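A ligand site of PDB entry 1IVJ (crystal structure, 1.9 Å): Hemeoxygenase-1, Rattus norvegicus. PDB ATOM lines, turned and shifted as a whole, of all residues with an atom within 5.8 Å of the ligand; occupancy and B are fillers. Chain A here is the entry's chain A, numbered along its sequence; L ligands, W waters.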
ATOM      1  N   SER A  14      16.583  -5.092  -5.613  1.00  0.00           N
ATOM      2  CA  SER A  14      15.274  -5.727  -5.756  1.00  0.00           C
ATOM      3  C   SER A  14      14.379  -5.452  -4.543  1.00  0.00           C
ATOM      4  O   SER A  14      13.195  -5.189  -4.692  1.00  0.00           O
ATOM      5  CB  SER A  14      15.432  -7.241  -5.946  1.00  0.00           C
ATOM      6  OG  SER A  14      15.966  -7.851  -4.782  1.00  0.00           O
ATOM      7  N   LEU A  17      13.465  -1.692  -4.470  1.00  0.00           N
ATOM      8  CA  LEU A  17      12.404  -1.385  -5.432  1.00  0.00           C
ATOM      9  C   LEU A  17      11.043  -1.829  -4.924  1.00  0.00           C
ATOM     10  O   LEU A  17      10.065  -1.090  -5.020  1.00  0.00           O
ATOM     11  CB  LEU A  17      12.697  -2.045  -6.784  1.00  0.00           C
ATOM     12  CG  LEU A  17      13.695  -1.322  -7.686  1.00  0.00           C
ATOM     13  CD1 LEU A  17      14.026  -2.184  -8.887  1.00  0.00           C
ATOM     14  CD2 LEU A  17      13.109   0.021  -8.133  1.00  0.00           C
ATOM     15  N   LYS A  18      10.976  -3.053  -4.395  1.00  0.00           N
ATOM     16  CA  LYS A  18       9.706  -3.562  -3.875  1.00  0.00           C
ATOM     17  C   LYS A  18       9.197  -2.634  -2.769  1.00  0.00           C
ATOM     18  O   LYS A  18       8.022  -2.254  -2.759  1.00  0.00           O
ATOM     19  CB  LYS A  18       9.874  -4.977  -3.315  1.00  0.00           C
ATOM     20  CG  LYS A  18       8.579  -5.566  -2.763  1.00  0.00           C
ATOM     21  CD  LYS A  18       8.807  -6.992  -2.260  1.00  0.00           C
ATOM     22  CE  LYS A  18       7.533  -7.589  -1.697  1.00  0.00           C
ATOM     23  NZ  LYS A  18       6.445  -7.654  -2.704  1.00  0.00           N
ATOM     24  N   THR A  21       8.088   0.925  -4.136  1.00  0.00           N
ATOM     25  CA  THR A  21       6.878   0.976  -4.932  1.00  0.00           C
ATOM     26  C   THR A  21       5.658   0.250  -4.363  1.00  0.00           C
ATOM     27  O   THR A  21       4.601   0.252  -4.994  1.00  0.00           O
ATOM     28  CB  THR A  21       7.135   0.420  -6.358  1.00  0.00           C
ATOM     29  OG1 THR A  21       7.500  -0.967  -6.268  1.00  0.00           O
ATOM     30  CG2 THR A  21       8.263   1.183  -7.030  1.00  0.00           C
ATOM     31  N   HIS A  25       1.907   0.955  -5.749  1.00  0.00           N
ATOM     32  CA  HIS A  25       1.383  -0.225  -6.436  1.00  0.00           C
ATOM     33  C   HIS A  25      -0.068  -0.420  -6.007  1.00  0.00           C
ATOM     34  O   HIS A  25      -0.930  -0.743  -6.818  1.00  0.00           O
ATOM     35  CB  HIS A  25       2.189  -1.480  -6.092  1.00  0.00           C
ATOM     36  CG  HIS A  25       1.692  -2.716  -6.781  1.00  0.00           C
ATOM     37  ND1 HIS A  25       0.564  -3.406  -6.356  1.00  0.00           N
ATOM     38  CD2 HIS A  25       2.115  -3.351  -7.903  1.00  0.00           C
ATOM     39  CE1 HIS A  25       0.334  -4.411  -7.187  1.00  0.00           C
ATOM     40  NE2 HIS A  25       1.250  -4.391  -8.139  1.00  0.00           N
ATOM     41  N   ALA A  28      -2.133   1.943  -7.814  1.00  0.00           N
ATOM     42  CA  ALA A  28      -2.248   1.599  -9.228  1.00  0.00           C
ATOM     43  C   ALA A  28      -3.204   0.415  -9.418  1.00  0.00           C
ATOM     44  O   ALA A  28      -4.099   0.478 -10.266  1.00  0.00           O
ATOM     45  CB  ALA A  28      -0.872   1.252  -9.797  1.00  0.00           C
ATOM     46  N   GLU A  29      -3.019  -0.639  -8.643  1.00  0.00           N
ATOM     47  CA  GLU A  29      -3.872  -1.823  -8.746  1.00  0.00           C
ATOM     48  C   GLU A  29      -5.328  -1.494  -8.424  1.00  0.00           C
ATOM     49  O   GLU A  29      -6.240  -2.203  -8.841  1.00  0.00           O
ATOM     50  CB  GLU A  29      -3.364  -2.927  -7.806  1.00  0.00           C
ATOM     51  CG  GLU A  29      -4.473  -3.700  -7.094  1.00  0.00           C
ATOM     52  CD  GLU A  29      -4.018  -5.059  -6.585  1.00  0.00           C
ATOM     53  OE1 GLU A  29      -2.877  -5.160  -6.097  1.00  0.00           O
ATOM     54  OE2 GLU A  29      -4.820  -6.013  -6.641  1.00  0.00           O
ATOM     55  N   ASN A  30      -5.531  -0.420  -7.673  1.00  0.00           N
ATOM     56  CA  ASN A  30      -6.875  -0.026  -7.290  1.00  0.00           C
ATOM     57  C   ASN A  30      -7.391   1.194  -8.052  1.00  0.00           C
ATOM     58  O   ASN A  30      -8.337   1.847  -7.610  1.00  0.00           O
ATOM     59  CB  ASN A  30      -6.930   0.223  -5.781  1.00  0.00           C
ATOM     60  CG  ASN A  30      -6.878  -1.070  -4.989  1.00  0.00           C
ATOM     61  OD1 ASN A  30      -7.852  -1.830  -4.952  1.00  0.00           O
ATOM     62  ND2 ASN A  30      -5.741  -1.342  -4.372  1.00  0.00           N
ATOM     63  N   MET A  34      -8.568  -0.100 -13.630  1.00  0.00           N
ATOM     64  CA  MET A  34      -8.177  -1.450 -13.235  1.00  0.00           C
ATOM     65  C   MET A  34      -9.236  -2.107 -12.362  1.00  0.00           C
ATOM     66  O   MET A  34      -9.474  -3.308 -12.463  1.00  0.00           O
ATOM     67  CB  MET A  34      -6.851  -1.430 -12.478  1.00  0.00           C
ATOM     68  CG  MET A  34      -5.645  -1.214 -13.361  1.00  0.00           C
ATOM     69  SD  MET A  34      -5.565  -2.470 -14.652  1.00  0.00           S
ATOM     70  CE  MET A  34      -5.858  -1.500 -16.081  1.00  0.00           C
ATOM     71  N   GLN A  38     -10.798  -5.562 -13.314  1.00  0.00           N
ATOM     72  CA  GLN A  38     -10.813  -6.700 -12.395  1.00  0.00           C
ATOM     73  C   GLN A  38     -12.228  -7.179 -12.083  1.00  0.00           C
ATOM     74  O   GLN A  38     -12.415  -8.310 -11.654  1.00  0.00           O
ATOM     75  CB  GLN A  38     -10.075  -6.350 -11.108  1.00  0.00           C
ATOM     76  CG  GLN A  38      -8.598  -6.006 -11.315  1.00  0.00           C
ATOM     77  CD  GLN A  38      -7.895  -5.634 -10.028  1.00  0.00           C
ATOM     78  OE1 GLN A  38      -7.697  -6.482  -9.148  1.00  0.00           O
ATOM     79  NE2 GLN A  38      -7.508  -4.373  -9.905  1.00  0.00           N
ATOM     80  N   TYR A 114       4.332   9.451 -21.333  1.00  0.00           N
ATOM     81  CA  TYR A 114       5.048   8.261 -20.869  1.00  0.00           C
ATOM     82  C   TYR A 114       6.213   7.993 -21.826  1.00  0.00           C
ATOM     83  O   TYR A 114       7.357   7.855 -21.411  1.00  0.00           O
ATOM     84  CB  TYR A 114       4.083   7.065 -20.879  1.00  0.00           C
ATOM     85  CG  TYR A 114       4.451   5.882 -20.002  1.00  0.00           C
ATOM     86  CD1 TYR A 114       5.786   5.515 -19.812  1.00  0.00           C
ATOM     87  CD2 TYR A 114       3.464   5.076 -19.457  1.00  0.00           C
ATOM     88  CE1 TYR A 114       6.114   4.364 -19.096  1.00  0.00           C
ATOM     89  CE2 TYR A 114       3.778   3.925 -18.741  1.00  0.00           C
ATOM     90  CZ  TYR A 114       5.100   3.573 -18.561  1.00  0.00           C
ATOM     91  OH  TYR A 114       5.402   2.425 -17.886  1.00  0.00           O
ATOM     92  N   TYR A 134      11.569  -2.844 -15.067  1.00  0.00           N
ATOM     93  CA  TYR A 134      11.073  -3.475 -13.851  1.00  0.00           C
ATOM     94  C   TYR A 134       9.574  -3.243 -13.667  1.00  0.00           C
ATOM     95  O   TYR A 134       8.794  -4.178 -13.480  1.00  0.00           O
ATOM     96  CB  TYR A 134      11.827  -2.900 -12.648  1.00  0.00           C
ATOM     97  CG  TYR A 134      11.107  -3.083 -11.314  1.00  0.00           C
ATOM     98  CD1 TYR A 134      11.119  -4.316 -10.661  1.00  0.00           C
ATOM     99  CD2 TYR A 134      10.452  -2.013 -10.709  1.00  0.00           C
ATOM    100  CE1 TYR A 134      10.490  -4.479  -9.432  1.00  0.00           C
ATOM    101  CE2 TYR A 134       9.816  -2.168  -9.480  1.00  0.00           C
ATOM    102  CZ  TYR A 134       9.842  -3.402  -8.835  1.00  0.00           C
ATOM    103  OH  TYR A 134       9.262  -3.544  -7.602  1.00  0.00           O
ATOM    104  N   THR A 135       9.184  -1.978 -13.727  1.00  0.00           N
ATOM    105  CA  THR A 135       7.786  -1.592 -13.538  1.00  0.00           C
ATOM    106  C   THR A 135       6.820  -2.249 -14.517  1.00  0.00           C
ATOM    107  O   THR A 135       5.769  -2.754 -14.116  1.00  0.00           O
ATOM    108  CB  THR A 135       7.637  -0.054 -13.618  1.00  0.00           C
ATOM    109  OG1 THR A 135       8.385   0.545 -12.554  1.00  0.00           O
ATOM    110  CG2 THR A 135       6.164   0.343 -13.472  1.00  0.00           C
ATOM    111  N   ARG A 136       7.172  -2.270 -15.804  1.00  0.00           N
ATOM    112  CA  ARG A 136       6.270  -2.893 -16.767  1.00  0.00           C
ATOM    113  C   ARG A 136       6.377  -4.415 -16.830  1.00  0.00           C
ATOM    114  O   ARG A 136       5.395  -5.116 -16.598  1.00  0.00           O
ATOM    115  CB  ARG A 136       6.478  -2.301 -18.173  1.00  0.00           C
ATOM    116  CG  ARG A 136       5.879  -0.902 -18.386  1.00  0.00           C
ATOM    117  CD  ARG A 136       4.408  -0.812 -17.990  1.00  0.00           C
ATOM    118  NE  ARG A 136       3.603  -1.945 -18.459  1.00  0.00           N
ATOM    119  CZ  ARG A 136       2.294  -2.085 -18.269  1.00  0.00           C
ATOM    120  NH1 ARG A 136       1.612  -1.139 -17.613  1.00  0.00           N
ATOM    121  NH2 ARG A 136       1.658  -3.166 -18.695  1.00  0.00           N
ATOM    122  N   LEU A 138       7.801  -6.858 -14.832  1.00  0.00           N
ATOM    123  CA  LEU A 138       7.453  -7.652 -13.668  1.00  0.00           C
ATOM    124  C   LEU A 138       5.952  -7.603 -13.397  1.00  0.00           C
ATOM    125  O   LEU A 138       5.381  -8.563 -12.878  1.00  0.00           O
ATOM    126  CB  LEU A 138       8.246  -7.221 -12.443  1.00  0.00           C
ATOM    127  CG  LEU A 138       9.759  -7.469 -12.496  1.00  0.00           C
ATOM    128  CD1 LEU A 138      10.243  -7.852 -11.099  1.00  0.00           C
ATOM    129  CD2 LEU A 138      10.094  -8.594 -13.473  1.00  0.00           C
ATOM    130  N   GLY A 139       5.328  -6.492 -13.750  1.00  0.00           N
ATOM    131  CA  GLY A 139       3.889  -6.368 -13.561  1.00  0.00           C
ATOM    132  C   GLY A 139       3.165  -7.277 -14.533  1.00  0.00           C
ATOM    133  O   GLY A 139       2.171  -7.921 -14.188  1.00  0.00           O
ATOM    134  N   ASP A 140       3.663  -7.324 -15.773  1.00  0.00           N
ATOM    135  CA  ASP A 140       3.093  -8.168 -16.812  1.00  0.00           C
ATOM    136  C   ASP A 140       3.090  -9.622 -16.365  1.00  0.00           C
ATOM    137  O   ASP A 140       2.163 -10.374 -16.665  1.00  0.00           O
ATOM    138  CB  ASP A 140       3.902  -8.054 -18.105  1.00  0.00           C
ATOM    139  CG  ASP A 140       3.849  -6.667 -18.711  1.00  0.00           C
ATOM    140  OD1 ASP A 140       4.735  -6.330 -19.523  1.00  0.00           O
ATOM    141  OD2 ASP A 140       2.896  -5.922 -18.374  1.00  0.00           O
ATOM    142  N   SER A 142       2.899 -10.647 -13.331  1.00  0.00           N
ATOM    143  CA  SER A 142       2.198 -10.782 -12.073  1.00  0.00           C
ATOM    144  C   SER A 142       0.714 -10.475 -12.286  1.00  0.00           C
ATOM    145  O   SER A 142      -0.044 -11.326 -12.724  1.00  0.00           O
ATOM    146  CB  SER A 142       2.821  -9.832 -11.044  1.00  0.00           C
ATOM    147  OG  SER A 142       4.216 -10.099 -10.884  1.00  0.00           O
ATOM    148  N   GLY A 143       0.304  -9.248 -11.978  1.00  0.00           N
ATOM    149  CA  GLY A 143      -1.081  -8.887 -12.161  1.00  0.00           C
ATOM    150  C   GLY A 143      -1.530  -9.011 -13.609  1.00  0.00           C
ATOM    151  O   GLY A 143      -2.702  -9.237 -13.879  1.00  0.00           O
ATOM    152  N   GLY A 144      -0.598  -8.866 -14.542  1.00  0.00           N
ATOM    153  CA  GLY A 144      -0.936  -8.981 -15.943  1.00  0.00           C
ATOM    154  C   GLY A 144      -1.534 -10.347 -16.255  1.00  0.00           C
ATOM    155  O   GLY A 144      -2.412 -10.476 -17.105  1.00  0.00           O
ATOM    156  N   VAL A 146      -3.314 -12.074 -14.227  1.00  0.00           N
ATOM    157  CA  VAL A 146      -4.662 -12.103 -13.671  1.00  0.00           C
ATOM    158  C   VAL A 146      -5.593 -11.379 -14.649  1.00  0.00           C
ATOM    159  O   VAL A 146      -6.707 -11.839 -14.911  1.00  0.00           O
ATOM    160  CB  VAL A 146      -4.721 -11.412 -12.305  1.00  0.00           C
ATOM    161  CG1 VAL A 146      -6.160 -11.291 -11.844  1.00  0.00           C
ATOM    162  CG2 VAL A 146      -3.921 -12.222 -11.289  1.00  0.00           C
ATOM    163  N   LEU A 147      -5.125 -10.253 -15.172  1.00  0.00           N
ATOM    164  CA  LEU A 147      -5.915  -9.476 -16.129  1.00  0.00           C
ATOM    165  C   LEU A 147      -6.182 -10.289 -17.391  1.00  0.00           C
ATOM    166  O   LEU A 147      -7.261 -10.198 -17.966  1.00  0.00           O
ATOM    167  CB  LEU A 147      -5.160  -8.201 -16.517  1.00  0.00           C
ATOM    168  CG  LEU A 147      -4.931  -7.187 -15.395  1.00  0.00           C
ATOM    169  CD1 LEU A 147      -4.052  -6.055 -15.915  1.00  0.00           C
ATOM    170  CD2 LEU A 147      -6.271  -6.651 -14.912  1.00  0.00           C
ATOM    171  N   LYS A 179      10.772 -14.260 -12.508  1.00  0.00           N
ATOM    172  CA  LYS A 179      10.811 -13.037 -11.715  1.00  0.00           C
ATOM    173  C   LYS A 179      11.906 -13.118 -10.656  1.00  0.00           C
ATOM    174  O   LYS A 179      12.606 -12.139 -10.403  1.00  0.00           O
ATOM    175  CB  LYS A 179       9.442 -12.781 -11.071  1.00  0.00           C
ATOM    176  CG  LYS A 179       8.386 -12.287 -12.060  1.00  0.00           C
ATOM    177  CD  LYS A 179       7.075 -11.907 -11.375  1.00  0.00           C
ATOM    178  CE  LYS A 179       6.310 -13.124 -10.894  1.00  0.00           C
ATOM    179  NZ  LYS A 179       5.094 -12.736 -10.133  1.00  0.00           N
ATOM    180  N   ARG A 183      14.937 -10.530 -10.341  1.00  0.00           N
ATOM    181  CA  ARG A 183      15.248  -9.771  -9.131  1.00  0.00           C
ATOM    182  C   ARG A 183      16.703  -9.998  -8.744  1.00  0.00           C
ATOM    183  O   ARG A 183      17.425  -9.069  -8.393  1.00  0.00           O
ATOM    184  CB  ARG A 183      14.348 -10.209  -7.964  1.00  0.00           C
ATOM    185  CG  ARG A 183      12.857  -9.936  -8.189  1.00  0.00           C
ATOM    186  CD  ARG A 183      12.040 -10.197  -6.917  1.00  0.00           C
ATOM    187  NE  ARG A 183      10.612 -10.015  -7.174  1.00  0.00           N
ATOM    188  CZ  ARG A 183       9.768 -10.979  -7.504  1.00  0.00           C
ATOM    189  NH1 ARG A 183      10.195 -12.233  -7.622  1.00  0.00           N
ATOM    190  NH2 ARG A 183       8.499 -10.700  -7.766  1.00  0.00           N
ATOM    191  N   PHE A 207       5.385   4.189 -12.052  1.00  0.00           N
ATOM    192  CA  PHE A 207       4.063   3.784 -11.589  1.00  0.00           C
ATOM    193  C   PHE A 207       3.055   4.912 -11.792  1.00  0.00           C
ATOM    194  O   PHE A 207       1.925   4.660 -12.202  1.00  0.00           O
ATOM    195  CB  PHE A 207       4.096   3.368 -10.119  1.00  0.00           C
ATOM    196  CG  PHE A 207       4.324   1.890  -9.901  1.00  0.00           C
ATOM    197  CD1 PHE A 207       5.613   1.368  -9.833  1.00  0.00           C
ATOM    198  CD2 PHE A 207       3.237   1.020  -9.776  1.00  0.00           C
ATOM    199  CE1 PHE A 207       5.816   0.005  -9.630  1.00  0.00           C
ATOM    200  CE2 PHE A 207       3.426  -0.343  -9.573  1.00  0.00           C
ATOM    201  CZ  PHE A 207       4.722  -0.857  -9.505  1.00  0.00           C
ATOM    202  N   ASN A 210       1.806   5.276 -15.300  1.00  0.00           N
ATOM    203  CA  ASN A 210       0.804   4.271 -15.601  1.00  0.00           C
ATOM    204  C   ASN A 210      -0.538   4.679 -15.006  1.00  0.00           C
ATOM    205  O   ASN A 210      -1.574   4.576 -15.662  1.00  0.00           O
ATOM    206  CB  ASN A 210       1.229   2.909 -15.053  1.00  0.00           C
ATOM    207  CG  ASN A 210       2.227   2.216 -15.967  1.00  0.00           C
ATOM    208  OD1 ASN A 210       1.859   1.622 -16.969  1.00  0.00           O
ATOM    209  ND2 ASN A 210       3.507   2.307 -15.619  1.00  0.00           N
ATOM    210  N   PHE A 214      -4.105   5.332 -17.047  1.00  0.00           N
ATOM    211  CA  PHE A 214      -5.389   4.714 -16.716  1.00  0.00           C
ATOM    212  C   PHE A 214      -6.449   5.744 -16.367  1.00  0.00           C
ATOM    213  O   PHE A 214      -7.607   5.604 -16.761  1.00  0.00           O
ATOM    214  CB  PHE A 214      -5.230   3.728 -15.557  1.00  0.00           C
ATOM    215  CG  PHE A 214      -4.301   2.585 -15.861  1.00  0.00           C
ATOM    216  CD1 PHE A 214      -4.407   1.886 -17.056  1.00  0.00           C
ATOM    217  CD2 PHE A 214      -3.339   2.197 -14.940  1.00  0.00           C
ATOM    218  CE1 PHE A 214      -3.548   0.828 -17.348  1.00  0.00           C
ATOM    219  CE2 PHE A 214      -2.473   1.145 -15.221  1.00  0.00           C
ATOM    220  CZ  PHE A 214      -2.578   0.461 -16.425  1.00  0.00           C
HETATM  221  C1  LIG L   1       3.796  -7.352  -8.371  1.00  0.00           C
HETATM  222  C2  LIG L   1      -0.993  -7.842  -8.676  1.00  0.00           C
HETATM  223  C3  LIG L   1      -1.210  -3.674 -11.118  1.00  0.00           C
HETATM  224  C4  LIG L   1       3.562  -3.623 -11.464  1.00  0.00           C
HETATM  225  C5  LIG L   1       2.508  -7.846  -8.193  1.00  0.00           C
HETATM  226  C6  LIG L   1       2.174  -9.025  -7.414  1.00  0.00           C
HETATM  227  C7  LIG L   1       0.823  -9.188  -7.519  1.00  0.00           C
HETATM  228  C8  LIG L   1       0.338  -8.062  -8.346  1.00  0.00           C
HETATM  229  C9  LIG L   1      -0.051 -10.274  -6.945  1.00  0.00           C
HETATM  230  C10 LIG L   1       3.155  -9.894  -6.624  1.00  0.00           C
HETATM  231  C11 LIG L   1       4.032 -10.872  -7.492  1.00  0.00           C
HETATM  232  C12 LIG L   1       5.185 -11.435  -6.873  1.00  0.00           C
HETATM  233  O1  LIG L   1       5.979 -12.105  -7.655  1.00  0.00           O
HETATM  234  O2  LIG L   1       5.469 -11.314  -5.655  1.00  0.00           O
HETATM  235  C13 LIG L   1      -1.459  -6.796  -9.487  1.00  0.00           C
HETATM  236  C14 LIG L   1      -2.842  -6.666  -9.937  1.00  0.00           C
HETATM  237  C15 LIG L   1      -2.927  -5.448 -10.535  1.00  0.00           C
HETATM  238  C16 LIG L   1      -1.569  -4.902 -10.565  1.00  0.00           C
HETATM  239  C17 LIG L   1      -3.915  -7.717  -9.743  1.00  0.00           C
HETATM  240  C18 LIG L   1      -4.152  -4.761 -11.090  1.00  0.00           C
HETATM  241  C19 LIG L   1      -4.277  -4.878 -12.620  1.00  0.00           C
HETATM  242  C20 LIG L   1       0.055  -3.296 -11.455  1.00  0.00           C
HETATM  243  C21 LIG L   1       0.391  -2.142 -12.275  1.00  0.00           C
HETATM  244  C22 LIG L   1       1.740  -2.118 -12.330  1.00  0.00           C
HETATM  245  C23 LIG L   1       2.231  -3.266 -11.605  1.00  0.00           C
HETATM  246  C24 LIG L   1      -0.633  -1.206 -12.904  1.00  0.00           C
HETATM  247  C25 LIG L   1       2.639  -1.036 -12.963  1.00  0.00           C
HETATM  248  C26 LIG L   1       2.532  -1.023 -14.524  1.00  0.00           C
HETATM  249  C27 LIG L   1       4.068  -4.589 -10.575  1.00  0.00           C
HETATM  250  C28 LIG L   1       5.486  -4.781 -10.279  1.00  0.00           C
HETATM  251  C29 LIG L   1       5.549  -5.870  -9.473  1.00  0.00           C
HETATM  252  C30 LIG L   1       4.159  -6.283  -9.205  1.00  0.00           C
HETATM  253  C31 LIG L   1       6.581  -3.898 -10.824  1.00  0.00           C
HETATM  254  C32 LIG L   1       6.743  -6.600  -8.902  1.00  0.00           C
HETATM  255  C33 LIG L   1       7.121  -6.099  -7.444  1.00  0.00           C
HETATM  256  C34 LIG L   1       8.270  -6.733  -6.930  1.00  0.00           C
HETATM  257  O3  LIG L   1       9.296  -6.038  -6.648  1.00  0.00           O
HETATM  258  O4  LIG L   1       8.299  -7.973  -6.728  1.00  0.00           O
HETATM  259  N1  LIG L   1       1.388  -7.267  -8.739  1.00  0.00           N
HETATM  260  N2  LIG L   1      -0.676  -5.770  -9.980  1.00  0.00           N
HETATM  261  N3  LIG L   1       1.208  -3.981 -11.035  1.00  0.00           N
HETATM  262  N4  LIG L   1       3.276  -5.487  -9.874  1.00  0.00           N
HETATM  263 FE1  LIG L   1       1.305  -5.610  -9.881  1.00  0.00          FE
HETATM  264  O   HOH W   1       7.447 -13.057  -4.635  1.00  0.00           O
HETATM  265  O   HOH W   2       6.507 -14.595  -6.673  1.00  0.00           O
HETATM  266  O   HOH W   3      11.668  -7.037  -5.959  1.00  0.00           O
HETATM  267  O   HOH W   4       6.429  -8.768  -5.056  1.00  0.00           O
HETATM  268  O   HOH W   5       2.781  -6.337  -5.330  1.00  0.00           O
HETATM  269  O   HOH W   6       3.195  -3.832 -15.522  1.00  0.00           O
HETATM  270  O   HOH W   7       2.060 -13.174  -6.696  1.00  0.00           O
HETATM  271  O   HOH W   8       2.135 -12.736  -9.504  1.00  0.00           O
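OH of Tyr 134 sits at hydrogen-bond distance from OG1 of Thr 21 (3.4 Å). The side-chain hydroxyl (OG) of Ser 142 sits at hydrogen-bond distance from the side-chain amino group (NZ) of Lys 179. OD1 of Asn 210 sits at hydrogen-bond distance from NH1 of Arg 136, at 2.8 Å. The side-chain amide nitrogen (NE2) of Gln 38 sits close to the backbone carbonyl oxygen (O) of Met 34. The backbone carbonyl oxygen (O) of Gly 139 sits at hydrogen-bond distance from the backbone NH (N) of Gly 144, at 2.9 Å. The backbone carbonyl oxygen of Leu 138 is in hydrogen-bond range of the side-chain hydroxyl of Ser 142 (2.8 Å). The side-chain amide nitrogen (ND2) of Asn 210 lies within hydrogen-bond range of the side-chain hydroxyl (OH) of Tyr 114, 3.0 Å away. NE2 of Gln 38 is in hydrogen-bond range of O of Glu 29 (2.7 Å).
Merely in contact with the ligand: Arg 136, Met 34, Gly 143, Gly 139, Ser 142, Leu 147, Lys 18, Phe 207, Thr 135, Asn 210, Gln 38, Glu 29, Phe 214, Leu 138 and Ala 28. Of the 27 residues printed, 19 come within 4 Å of the ligand. Along chain A the residues within 4 Å of the ligand span positions 18 to 214.
Water W4 bridges the side-chain amino group of Lys 18 and an oxygen (O4) of the ligand. Water W3 lies within hydrogen-bond range of O3 of the ligand, O of Ser 14 and NE of Arg 183.
An iron atom (FE1) of the ligand is bound by a ring nitrogen (NE2) of His 25 (2.1 Å). The side-chain hydroxyl (OH) of Tyr 134 lies within hydrogen-bond range of an oxygen (O3) of the ligand, at 2.7 Å. An oxygen (O1) of the ligand is in salt-bridge range of the side-chain amino group (NZ) of Lys 179, 2.7 Å away. The guanidinium group of Arg 183 is in salt-bridge range of an oxygen (O1) of the ligand.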
